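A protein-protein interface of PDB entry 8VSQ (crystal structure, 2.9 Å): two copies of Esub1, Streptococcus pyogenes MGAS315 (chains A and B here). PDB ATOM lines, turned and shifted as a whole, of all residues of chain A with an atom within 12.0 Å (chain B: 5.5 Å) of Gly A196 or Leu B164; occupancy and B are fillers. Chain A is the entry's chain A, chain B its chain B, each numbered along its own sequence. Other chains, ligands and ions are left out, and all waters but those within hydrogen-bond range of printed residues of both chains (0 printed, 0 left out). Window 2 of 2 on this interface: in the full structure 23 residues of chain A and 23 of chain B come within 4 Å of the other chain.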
ATOM      1  N   TRP A 186       8.156  26.855 -24.519  1.00  0.00           N
ATOM      2  CA  TRP A 186       9.545  27.200 -24.911  1.00  0.00           C
ATOM      3  C   TRP A 186      10.312  27.717 -23.694  1.00  0.00           C
ATOM      4  O   TRP A 186      11.498  27.460 -23.609  1.00  0.00           O
ATOM      5  CB  TRP A 186       9.530  28.244 -26.032  1.00  0.00           C
ATOM      6  CG  TRP A 186      10.861  28.832 -26.382  1.00  0.00           C
ATOM      7  CD1 TRP A 186      11.177  30.152 -26.524  1.00  0.00           C
ATOM      8  CD2 TRP A 186      12.070  28.104 -26.667  1.00  0.00           C
ATOM      9  NE1 TRP A 186      12.485  30.298 -26.895  1.00  0.00           N
ATOM     10  CE2 TRP A 186      13.052  29.060 -26.991  1.00  0.00           C
ATOM     11  CE3 TRP A 186      12.397  26.741 -26.723  1.00  0.00           C
ATOM     12  CZ2 TRP A 186      14.351  28.684 -27.307  1.00  0.00           C
ATOM     13  CZ3 TRP A 186      13.674  26.377 -27.064  1.00  0.00           C
ATOM     14  CH2 TRP A 186      14.638  27.340 -27.339  1.00  0.00           C
ATOM     15  N   GLU A 187       9.658  28.453 -22.801  1.00  0.00           N
ATOM     16  CA  GLU A 187      10.304  28.991 -21.574  1.00  0.00           C
ATOM     17  C   GLU A 187      10.553  27.845 -20.607  1.00  0.00           C
ATOM     18  O   GLU A 187      11.434  27.989 -19.733  1.00  0.00           O
ATOM     19  CB  GLU A 187       9.448  30.021 -20.844  1.00  0.00           C
ATOM     20  CG  GLU A 187       9.425  31.351 -21.539  1.00  0.00           C
ATOM     21  CD  GLU A 187       8.524  32.380 -20.892  1.00  0.00           C
ATOM     22  OE1 GLU A 187       7.927  32.050 -19.835  1.00  0.00           O
ATOM     23  OE2 GLU A 187       8.432  33.511 -21.455  1.00  0.00           O
ATOM     24  N   TYR A 188       9.767  26.778 -20.712  1.00  0.00           N
ATOM     25  CA  TYR A 188       9.957  25.578 -19.878  1.00  0.00           C
ATOM     26  C   TYR A 188      11.217  24.850 -20.357  1.00  0.00           C
ATOM     27  O   TYR A 188      12.069  24.482 -19.521  1.00  0.00           O
ATOM     28  CB  TYR A 188       8.724  24.706 -19.932  1.00  0.00           C
ATOM     29  CG  TYR A 188       8.806  23.556 -18.977  1.00  0.00           C
ATOM     30  CD1 TYR A 188       9.434  22.372 -19.339  1.00  0.00           C
ATOM     31  CD2 TYR A 188       8.290  23.674 -17.699  1.00  0.00           C
ATOM     32  CE1 TYR A 188       9.517  21.312 -18.457  1.00  0.00           C
ATOM     33  CE2 TYR A 188       8.323  22.607 -16.820  1.00  0.00           C
ATOM     34  CZ  TYR A 188       8.947  21.432 -17.198  1.00  0.00           C
ATOM     35  OH  TYR A 188       8.980  20.418 -16.289  1.00  0.00           O
ATOM     36  N   ILE A 189      11.365  24.699 -21.668  1.00  0.00           N
ATOM     37  CA  ILE A 189      12.591  24.127 -22.286  1.00  0.00           C
ATOM     38  C   ILE A 189      13.816  24.983 -21.901  1.00  0.00           C
ATOM     39  O   ILE A 189      14.904  24.464 -21.540  1.00  0.00           O
ATOM     40  CB  ILE A 189      12.390  24.003 -23.805  1.00  0.00           C
ATOM     41  CG1 ILE A 189      11.786  22.647 -24.169  1.00  0.00           C
ATOM     42  CG2 ILE A 189      13.693  24.251 -24.551  1.00  0.00           C
ATOM     43  CD1 ILE A 189      10.399  22.418 -23.597  1.00  0.00           C
ATOM     44  N   GLN A 190      13.663  26.291 -21.967  1.00  0.00           N
ATOM     45  CA  GLN A 190      14.740  27.239 -21.603  1.00  0.00           C
ATOM     46  C   GLN A 190      15.127  26.954 -20.144  1.00  0.00           C
ATOM     47  O   GLN A 190      16.343  26.896 -19.869  1.00  0.00           O
ATOM     48  CB  GLN A 190      14.277  28.675 -21.896  1.00  0.00           C
ATOM     49  CG  GLN A 190      14.420  29.138 -23.355  1.00  0.00           C
ATOM     50  CD  GLN A 190      14.245  30.639 -23.492  1.00  0.00           C
ATOM     51  OE1 GLN A 190      15.137  31.435 -23.182  1.00  0.00           O
ATOM     52  NE2 GLN A 190      13.084  31.056 -23.969  1.00  0.00           N
ATOM     53  N   ASN A 191      14.152  26.723 -19.259  1.00  0.00           N
ATOM     54  CA  ASN A 191      14.419  26.474 -17.813  1.00  0.00           C
ATOM     55  C   ASN A 191      15.002  25.087 -17.633  1.00  0.00           C
ATOM     56  O   ASN A 191      15.696  24.880 -16.660  1.00  0.00           O
ATOM     57  CB  ASN A 191      13.193  26.695 -16.935  1.00  0.00           C
ATOM     58  CG  ASN A 191      12.796  28.149 -17.015  1.00  0.00           C
ATOM     59  OD1 ASN A 191      13.645  28.989 -17.324  1.00  0.00           O
ATOM     60  ND2 ASN A 191      11.522  28.446 -16.790  1.00  0.00           N
ATOM     61  N   GLU A 192      14.788  24.199 -18.581  1.00  0.00           N
ATOM     62  CA  GLU A 192      15.450  22.888 -18.514  1.00  0.00           C
ATOM     63  C   GLU A 192      16.941  23.154 -18.678  1.00  0.00           C
ATOM     64  O   GLU A 192      17.717  22.670 -17.839  1.00  0.00           O
ATOM     65  CB  GLU A 192      14.852  21.891 -19.510  1.00  0.00           C
ATOM     66  CG  GLU A 192      13.521  21.286 -19.038  1.00  0.00           C
ATOM     67  CD  GLU A 192      12.639  20.501 -20.080  1.00  0.00           C
ATOM     68  OE1 GLU A 192      12.884  20.643 -21.289  1.00  0.00           O
ATOM     69  OE2 GLU A 192      11.926  19.604 -19.576  1.00  0.00           O
ATOM     70  N   ILE A 193      17.319  23.944 -19.678  1.00  0.00           N
ATOM     71  CA  ILE A 193      18.748  24.296 -19.943  1.00  0.00           C
ATOM     72  C   ILE A 193      19.385  24.963 -18.709  1.00  0.00           C
ATOM     73  O   ILE A 193      20.388  24.428 -18.239  1.00  0.00           O
ATOM     74  CB  ILE A 193      18.861  25.175 -21.199  1.00  0.00           C
ATOM     75  CG1 ILE A 193      18.940  24.321 -22.468  1.00  0.00           C
ATOM     76  CG2 ILE A 193      20.054  26.138 -21.093  1.00  0.00           C
ATOM     77  CD1 ILE A 193      17.864  23.318 -22.625  1.00  0.00           C
ATOM     78  N   GLN A 194      18.820  26.071 -18.206  1.00  0.00           N
ATOM     79  CA  GLN A 194      19.319  26.842 -17.025  1.00  0.00           C
ATOM     80  C   GLN A 194      19.690  25.897 -15.870  1.00  0.00           C
ATOM     81  O   GLN A 194      20.799  26.064 -15.241  1.00  0.00           O
ATOM     82  CB  GLN A 194      18.263  27.855 -16.551  1.00  0.00           C
ATOM     83  CG  GLN A 194      18.036  29.015 -17.514  1.00  0.00           C
ATOM     84  CD  GLN A 194      19.343  29.670 -17.903  1.00  0.00           C
ATOM     85  OE1 GLN A 194      20.189  29.929 -17.049  1.00  0.00           O
ATOM     86  NE2 GLN A 194      19.551  29.884 -19.197  1.00  0.00           N
ATOM     87  N   LYS A 195      18.781  24.964 -15.582  1.00  0.00           N
ATOM     88  CA  LYS A 195      18.985  23.885 -14.587  1.00  0.00           C
ATOM     89  C   LYS A 195      20.149  23.012 -15.038  1.00  0.00           C
ATOM     90  O   LYS A 195      21.009  22.753 -14.189  1.00  0.00           O
ATOM     91  CB  LYS A 195      17.684  23.108 -14.408  1.00  0.00           C
ATOM     92  CG  LYS A 195      16.641  23.922 -13.659  1.00  0.00           C
ATOM     93  CD  LYS A 195      15.290  23.256 -13.480  1.00  0.00           C
ATOM     94  CE  LYS A 195      14.296  24.114 -12.715  1.00  0.00           C
ATOM     95  NZ  LYS A 195      12.913  23.567 -12.771  1.00  0.00           N
ATOM     96  N   GLY A 196      20.173  22.642 -16.326  1.00  0.00           N
ATOM     97  CA  GLY A 196      21.199  21.805 -16.986  1.00  0.00           C
ATOM     98  C   GLY A 196      22.618  22.278 -16.696  1.00  0.00           C
ATOM     99  O   GLY A 196      23.519  21.420 -16.519  1.00  0.00           O
ATOM    100  N   LEU A 197      22.833  23.591 -16.608  1.00  0.00           N
ATOM    101  CA  LEU A 197      24.155  24.138 -16.229  1.00  0.00           C
ATOM    102  C   LEU A 197      24.198  24.397 -14.720  1.00  0.00           C
ATOM    103  O   LEU A 197      25.291  24.416 -14.180  1.00  0.00           O
ATOM    104  CB  LEU A 197      24.460  25.375 -17.082  1.00  0.00           C
ATOM    105  CG  LEU A 197      23.388  26.450 -17.267  1.00  0.00           C
ATOM    106  CD1 LEU A 197      23.437  27.524 -16.196  1.00  0.00           C
ATOM    107  CD2 LEU A 197      23.604  27.089 -18.617  1.00  0.00           C
ATOM    108  N   GLY A 198      23.042  24.495 -14.054  1.00  0.00           N
ATOM    109  CA  GLY A 198      22.931  24.781 -12.605  1.00  0.00           C
ATOM    110  C   GLY A 198      24.268  24.787 -11.859  1.00  0.00           C
ATOM    111  O   GLY A 198      24.474  25.666 -10.994  1.00  0.00           O
ATOM    112  N   PHE B 120      23.963  30.316 -23.173  1.00  0.00           N
ATOM    113  CA  PHE B 120      23.151  29.824 -22.041  1.00  0.00           C
ATOM    114  C   PHE B 120      23.686  30.460 -20.767  1.00  0.00           C
ATOM    115  O   PHE B 120      22.859  30.943 -20.004  1.00  0.00           O
ATOM    116  CB  PHE B 120      23.056  28.298 -21.942  1.00  0.00           C
ATOM    117  CG  PHE B 120      22.553  27.606 -23.186  1.00  0.00           C
ATOM    118  CD1 PHE B 120      21.896  28.316 -24.189  1.00  0.00           C
ATOM    119  CD2 PHE B 120      22.759  26.245 -23.353  1.00  0.00           C
ATOM    120  CE1 PHE B 120      21.511  27.693 -25.358  1.00  0.00           C
ATOM    121  CE2 PHE B 120      22.383  25.624 -24.528  1.00  0.00           C
ATOM    122  CZ  PHE B 120      21.762  26.356 -25.521  1.00  0.00           C
ATOM    123  N   VAL B 159      30.315  17.170 -24.449  1.00  0.00           N
ATOM    124  CA  VAL B 159      29.245  16.195 -24.789  1.00  0.00           C
ATOM    125  C   VAL B 159      28.014  16.654 -24.032  1.00  0.00           C
ATOM    126  O   VAL B 159      26.964  16.500 -24.602  1.00  0.00           O
ATOM    127  CB  VAL B 159      29.618  14.727 -24.473  1.00  0.00           C
ATOM    128  CG1 VAL B 159      30.779  14.238 -25.356  1.00  0.00           C
ATOM    129  CG2 VAL B 159      29.932  14.492 -22.991  1.00  0.00           C
ATOM    130  N   LYS B 160      28.173  17.189 -22.815  1.00  0.00           N
ATOM    131  CA  LYS B 160      27.049  17.682 -21.977  1.00  0.00           C
ATOM    132  C   LYS B 160      26.696  19.062 -22.497  1.00  0.00           C
ATOM    133  O   LYS B 160      25.596  19.545 -22.217  1.00  0.00           O
ATOM    134  CB  LYS B 160      27.361  17.834 -20.490  1.00  0.00           C
ATOM    135  CG  LYS B 160      27.976  16.604 -19.832  1.00  0.00           C
ATOM    136  CD  LYS B 160      27.020  15.433 -19.471  1.00  0.00           C
ATOM    137  CE  LYS B 160      27.194  14.158 -20.290  1.00  0.00           C
ATOM    138  NZ  LYS B 160      25.914  13.404 -20.424  1.00  0.00           N
ATOM    139  N   GLN B 161      27.626  19.679 -23.212  1.00  0.00           N
ATOM    140  CA  GLN B 161      27.338  20.935 -23.905  1.00  0.00           C
ATOM    141  C   GLN B 161      26.518  20.580 -25.135  1.00  0.00           C
ATOM    142  O   GLN B 161      25.382  21.049 -25.189  1.00  0.00           O
ATOM    143  CB  GLN B 161      28.622  21.660 -24.269  1.00  0.00           C
ATOM    144  CG  GLN B 161      29.310  22.326 -23.085  1.00  0.00           C
ATOM    145  CD  GLN B 161      30.412  23.231 -23.597  1.00  0.00           C
ATOM    146  OE1 GLN B 161      30.214  24.099 -24.449  1.00  0.00           O
ATOM    147  NE2 GLN B 161      31.617  23.007 -23.115  1.00  0.00           N
ATOM    148  N   ASP B 162      27.054  19.775 -26.056  1.00  0.00           N
ATOM    149  CA  ASP B 162      26.393  19.533 -27.365  1.00  0.00           C
ATOM    150  C   ASP B 162      25.014  18.907 -27.147  1.00  0.00           C
ATOM    151  O   ASP B 162      24.163  18.965 -28.052  1.00  0.00           O
ATOM    152  CB  ASP B 162      27.258  18.668 -28.267  1.00  0.00           C
ATOM    153  CG  ASP B 162      28.571  19.363 -28.529  1.00  0.00           C
ATOM    154  OD1 ASP B 162      28.809  20.365 -27.860  1.00  0.00           O
ATOM    155  OD2 ASP B 162      29.315  18.915 -29.395  1.00  0.00           O
ATOM    156  N   TYR B 163      24.830  18.293 -25.990  1.00  0.00           N
ATOM    157  CA  TYR B 163      23.572  17.635 -25.603  1.00  0.00           C
ATOM    158  C   TYR B 163      22.585  18.753 -25.249  1.00  0.00           C
ATOM    159  O   TYR B 163      21.472  18.766 -25.773  1.00  0.00           O
ATOM    160  CB  TYR B 163      23.823  16.614 -24.489  1.00  0.00           C
ATOM    161  CG  TYR B 163      22.543  16.054 -23.944  1.00  0.00           C
ATOM    162  CD1 TYR B 163      21.912  15.017 -24.614  1.00  0.00           C
ATOM    163  CD2 TYR B 163      21.899  16.614 -22.843  1.00  0.00           C
ATOM    164  CE1 TYR B 163      20.697  14.500 -24.179  1.00  0.00           C
ATOM    165  CE2 TYR B 163      20.665  16.131 -22.411  1.00  0.00           C
ATOM    166  CZ  TYR B 163      20.065  15.050 -23.066  1.00  0.00           C
ATOM    167  OH  TYR B 163      18.866  14.514 -22.656  1.00  0.00           O
ATOM    168  N   LEU B 164      22.966  19.690 -24.396  1.00  0.00           N
ATOM    169  CA  LEU B 164      22.015  20.735 -23.942  1.00  0.00           C
ATOM    170  C   LEU B 164      21.679  21.715 -25.079  1.00  0.00           C
ATOM    171  O   LEU B 164      20.532  22.220 -25.137  1.00  0.00           O
ATOM    172  CB  LEU B 164      22.599  21.436 -22.716  1.00  0.00           C
ATOM    173  CG  LEU B 164      22.335  20.672 -21.428  1.00  0.00           C
ATOM    174  CD1 LEU B 164      22.128  21.611 -20.259  1.00  0.00           C
ATOM    175  CD2 LEU B 164      21.123  19.752 -21.571  1.00  0.00           C
ATOM    176  N   ILE B 165      22.631  21.964 -25.969  1.00  0.00           N
ATOM    177  CA  ILE B 165      22.382  22.736 -27.205  1.00  0.00           C
ATOM    178  C   ILE B 165      21.317  21.999 -27.989  1.00  0.00           C
ATOM    179  O   ILE B 165      20.301  22.612 -28.287  1.00  0.00           O
ATOM    180  CB  ILE B 165      23.661  22.924 -28.012  1.00  0.00           C
ATOM    181  CG1 ILE B 165      24.633  23.799 -27.223  1.00  0.00           C
ATOM    182  CG2 ILE B 165      23.337  23.469 -29.394  1.00  0.00           C
ATOM    183  CD1 ILE B 165      26.048  23.670 -27.732  1.00  0.00           C
ATOM    184  N   ASN B 166      21.492  20.716 -28.244  1.00  0.00           N
ATOM    185  CA  ASN B 166      20.462  19.973 -29.005  1.00  0.00           C
ATOM    186  C   ASN B 166      19.119  20.016 -28.309  1.00  0.00           C
ATOM    187  O   ASN B 166      18.168  20.282 -29.033  1.00  0.00           O
ATOM    188  CB  ASN B 166      20.837  18.547 -29.328  1.00  0.00           C
ATOM    189  CG  ASN B 166      21.344  18.561 -30.750  1.00  0.00           C
ATOM    190  OD1 ASN B 166      22.032  19.497 -31.164  1.00  0.00           O
ATOM    191  ND2 ASN B 166      20.941  17.584 -31.534  1.00  0.00           N
ATOM    192  N   HIS B 167      19.039  19.810 -26.994  1.00  0.00           N
ATOM    193  CA  HIS B 167      17.746  19.969 -26.280  1.00  0.00           C
ATOM    194  C   HIS B 167      17.141  21.339 -26.615  1.00  0.00           C
ATOM    195  O   HIS B 167      15.952  21.353 -27.040  1.00  0.00           O
ATOM    196  CB  HIS B 167      17.840  19.768 -24.776  1.00  0.00           C
ATOM    197  CG  HIS B 167      16.476  19.728 -24.161  1.00  0.00           C
ATOM    198  ND1 HIS B 167      15.622  18.641 -24.295  1.00  0.00           N
ATOM    199  CD2 HIS B 167      15.787  20.649 -23.446  1.00  0.00           C
ATOM    200  CE1 HIS B 167      14.469  18.920 -23.697  1.00  0.00           C
ATOM    201  NE2 HIS B 167      14.557  20.126 -23.135  1.00  0.00           N
ATOM    202  N   TYR B 168      17.929  22.419 -26.438  1.00  0.00           N
ATOM    203  CA  TYR B 168      17.565  23.827 -26.719  1.00  0.00           C
ATOM    204  C   TYR B 168      17.199  23.918 -28.193  1.00  0.00           C
ATOM    205  O   TYR B 168      16.095  24.311 -28.503  1.00  0.00           O
ATOM    206  CB  TYR B 168      18.703  24.774 -26.370  1.00  0.00           C
ATOM    207  CG  TYR B 168      18.465  26.229 -26.708  1.00  0.00           C
ATOM    208  CD1 TYR B 168      18.681  26.729 -27.990  1.00  0.00           C
ATOM    209  CD2 TYR B 168      18.045  27.102 -25.713  1.00  0.00           C
ATOM    210  CE1 TYR B 168      18.444  28.055 -28.280  1.00  0.00           C
ATOM    211  CE2 TYR B 168      17.804  28.427 -25.979  1.00  0.00           C
ATOM    212  CZ  TYR B 168      18.013  28.905 -27.257  1.00  0.00           C
ATOM    213  OH  TYR B 168      17.764  30.253 -27.360  1.00  0.00           O
ATOM    214  N   LEU B 169      18.073  23.537 -29.106  1.00  0.00           N
ATOM    215  CA  LEU B 169      17.760  23.792 -30.535  1.00  0.00           C
ATOM    216  C   LEU B 169      16.516  23.018 -30.930  1.00  0.00           C
ATOM    217  O   LEU B 169      15.843  23.514 -31.784  1.00  0.00           O
ATOM    218  CB  LEU B 169      18.931  23.451 -31.457  1.00  0.00           C
ATOM    219  CG  LEU B 169      20.037  24.509 -31.517  1.00  0.00           C
ATOM    220  CD1 LEU B 169      20.926  24.315 -32.739  1.00  0.00           C
ATOM    221  CD2 LEU B 169      19.469  25.933 -31.491  1.00  0.00           C
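OE1 of Glu A192 is in hydrogen-bond range of NE2 of His B167 (2.5 Å).
Tyr B168 touches Trp A186. Ile A189 touches His B167. Ile A193 touches Phe B120. CG1 of Ile A193 touches O of Leu B164, 3.8 Å away. Ile A193 touches His B167 (CD1 to CD2, 3.5 Å). Tyr B168 touches Ile A193 (N to CD1, 3.9 Å). Phe B120 touches Gln A194. CD1 of Leu B164 touches CA of Gly A196, at 3.4 Å. Phe B120 touches Leu A197.
No position is printed for both chains.
Gly A196 touches one residue of chain B. Leu B164 touches just these residues of chain A: Ile A193 and Gly A196. Tyr B163 touches none of the printed residues of chain A. No residue of chain A comes within 4 Å of Ile B165. His B167 touches three residues of chain A. Of the printed residues of chain A, Tyr B168 touches Trp A186 (3.5 Å) and Ile A193 (3.9 Å). Of the printed residues of chain B, Gln A194 touches Phe B120. Of the printed residues of chain B, Ile A189 touches His B167 (3.9 Å). Of the printed residues of chain B, Leu A197 touches Phe B120. Printed residues of chain B within 4 Å of Trp A186: Tyr B168 (3.5 Å). Lys A195 touches none of the printed residues of chain B. Glu A187 touches none of the printed residues of chain B. The nearest residue of chain A that does not touch Leu B164 is Leu A197 (4.2 Å).
Of the 12 printed residues of chain B, 4 touch a printed residue of chain A.
The indole nitrogen (NE1) of Trp A186 sits close to the side-chain amide nitrogen (NE2) of Gln A190 (3.1 Å).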
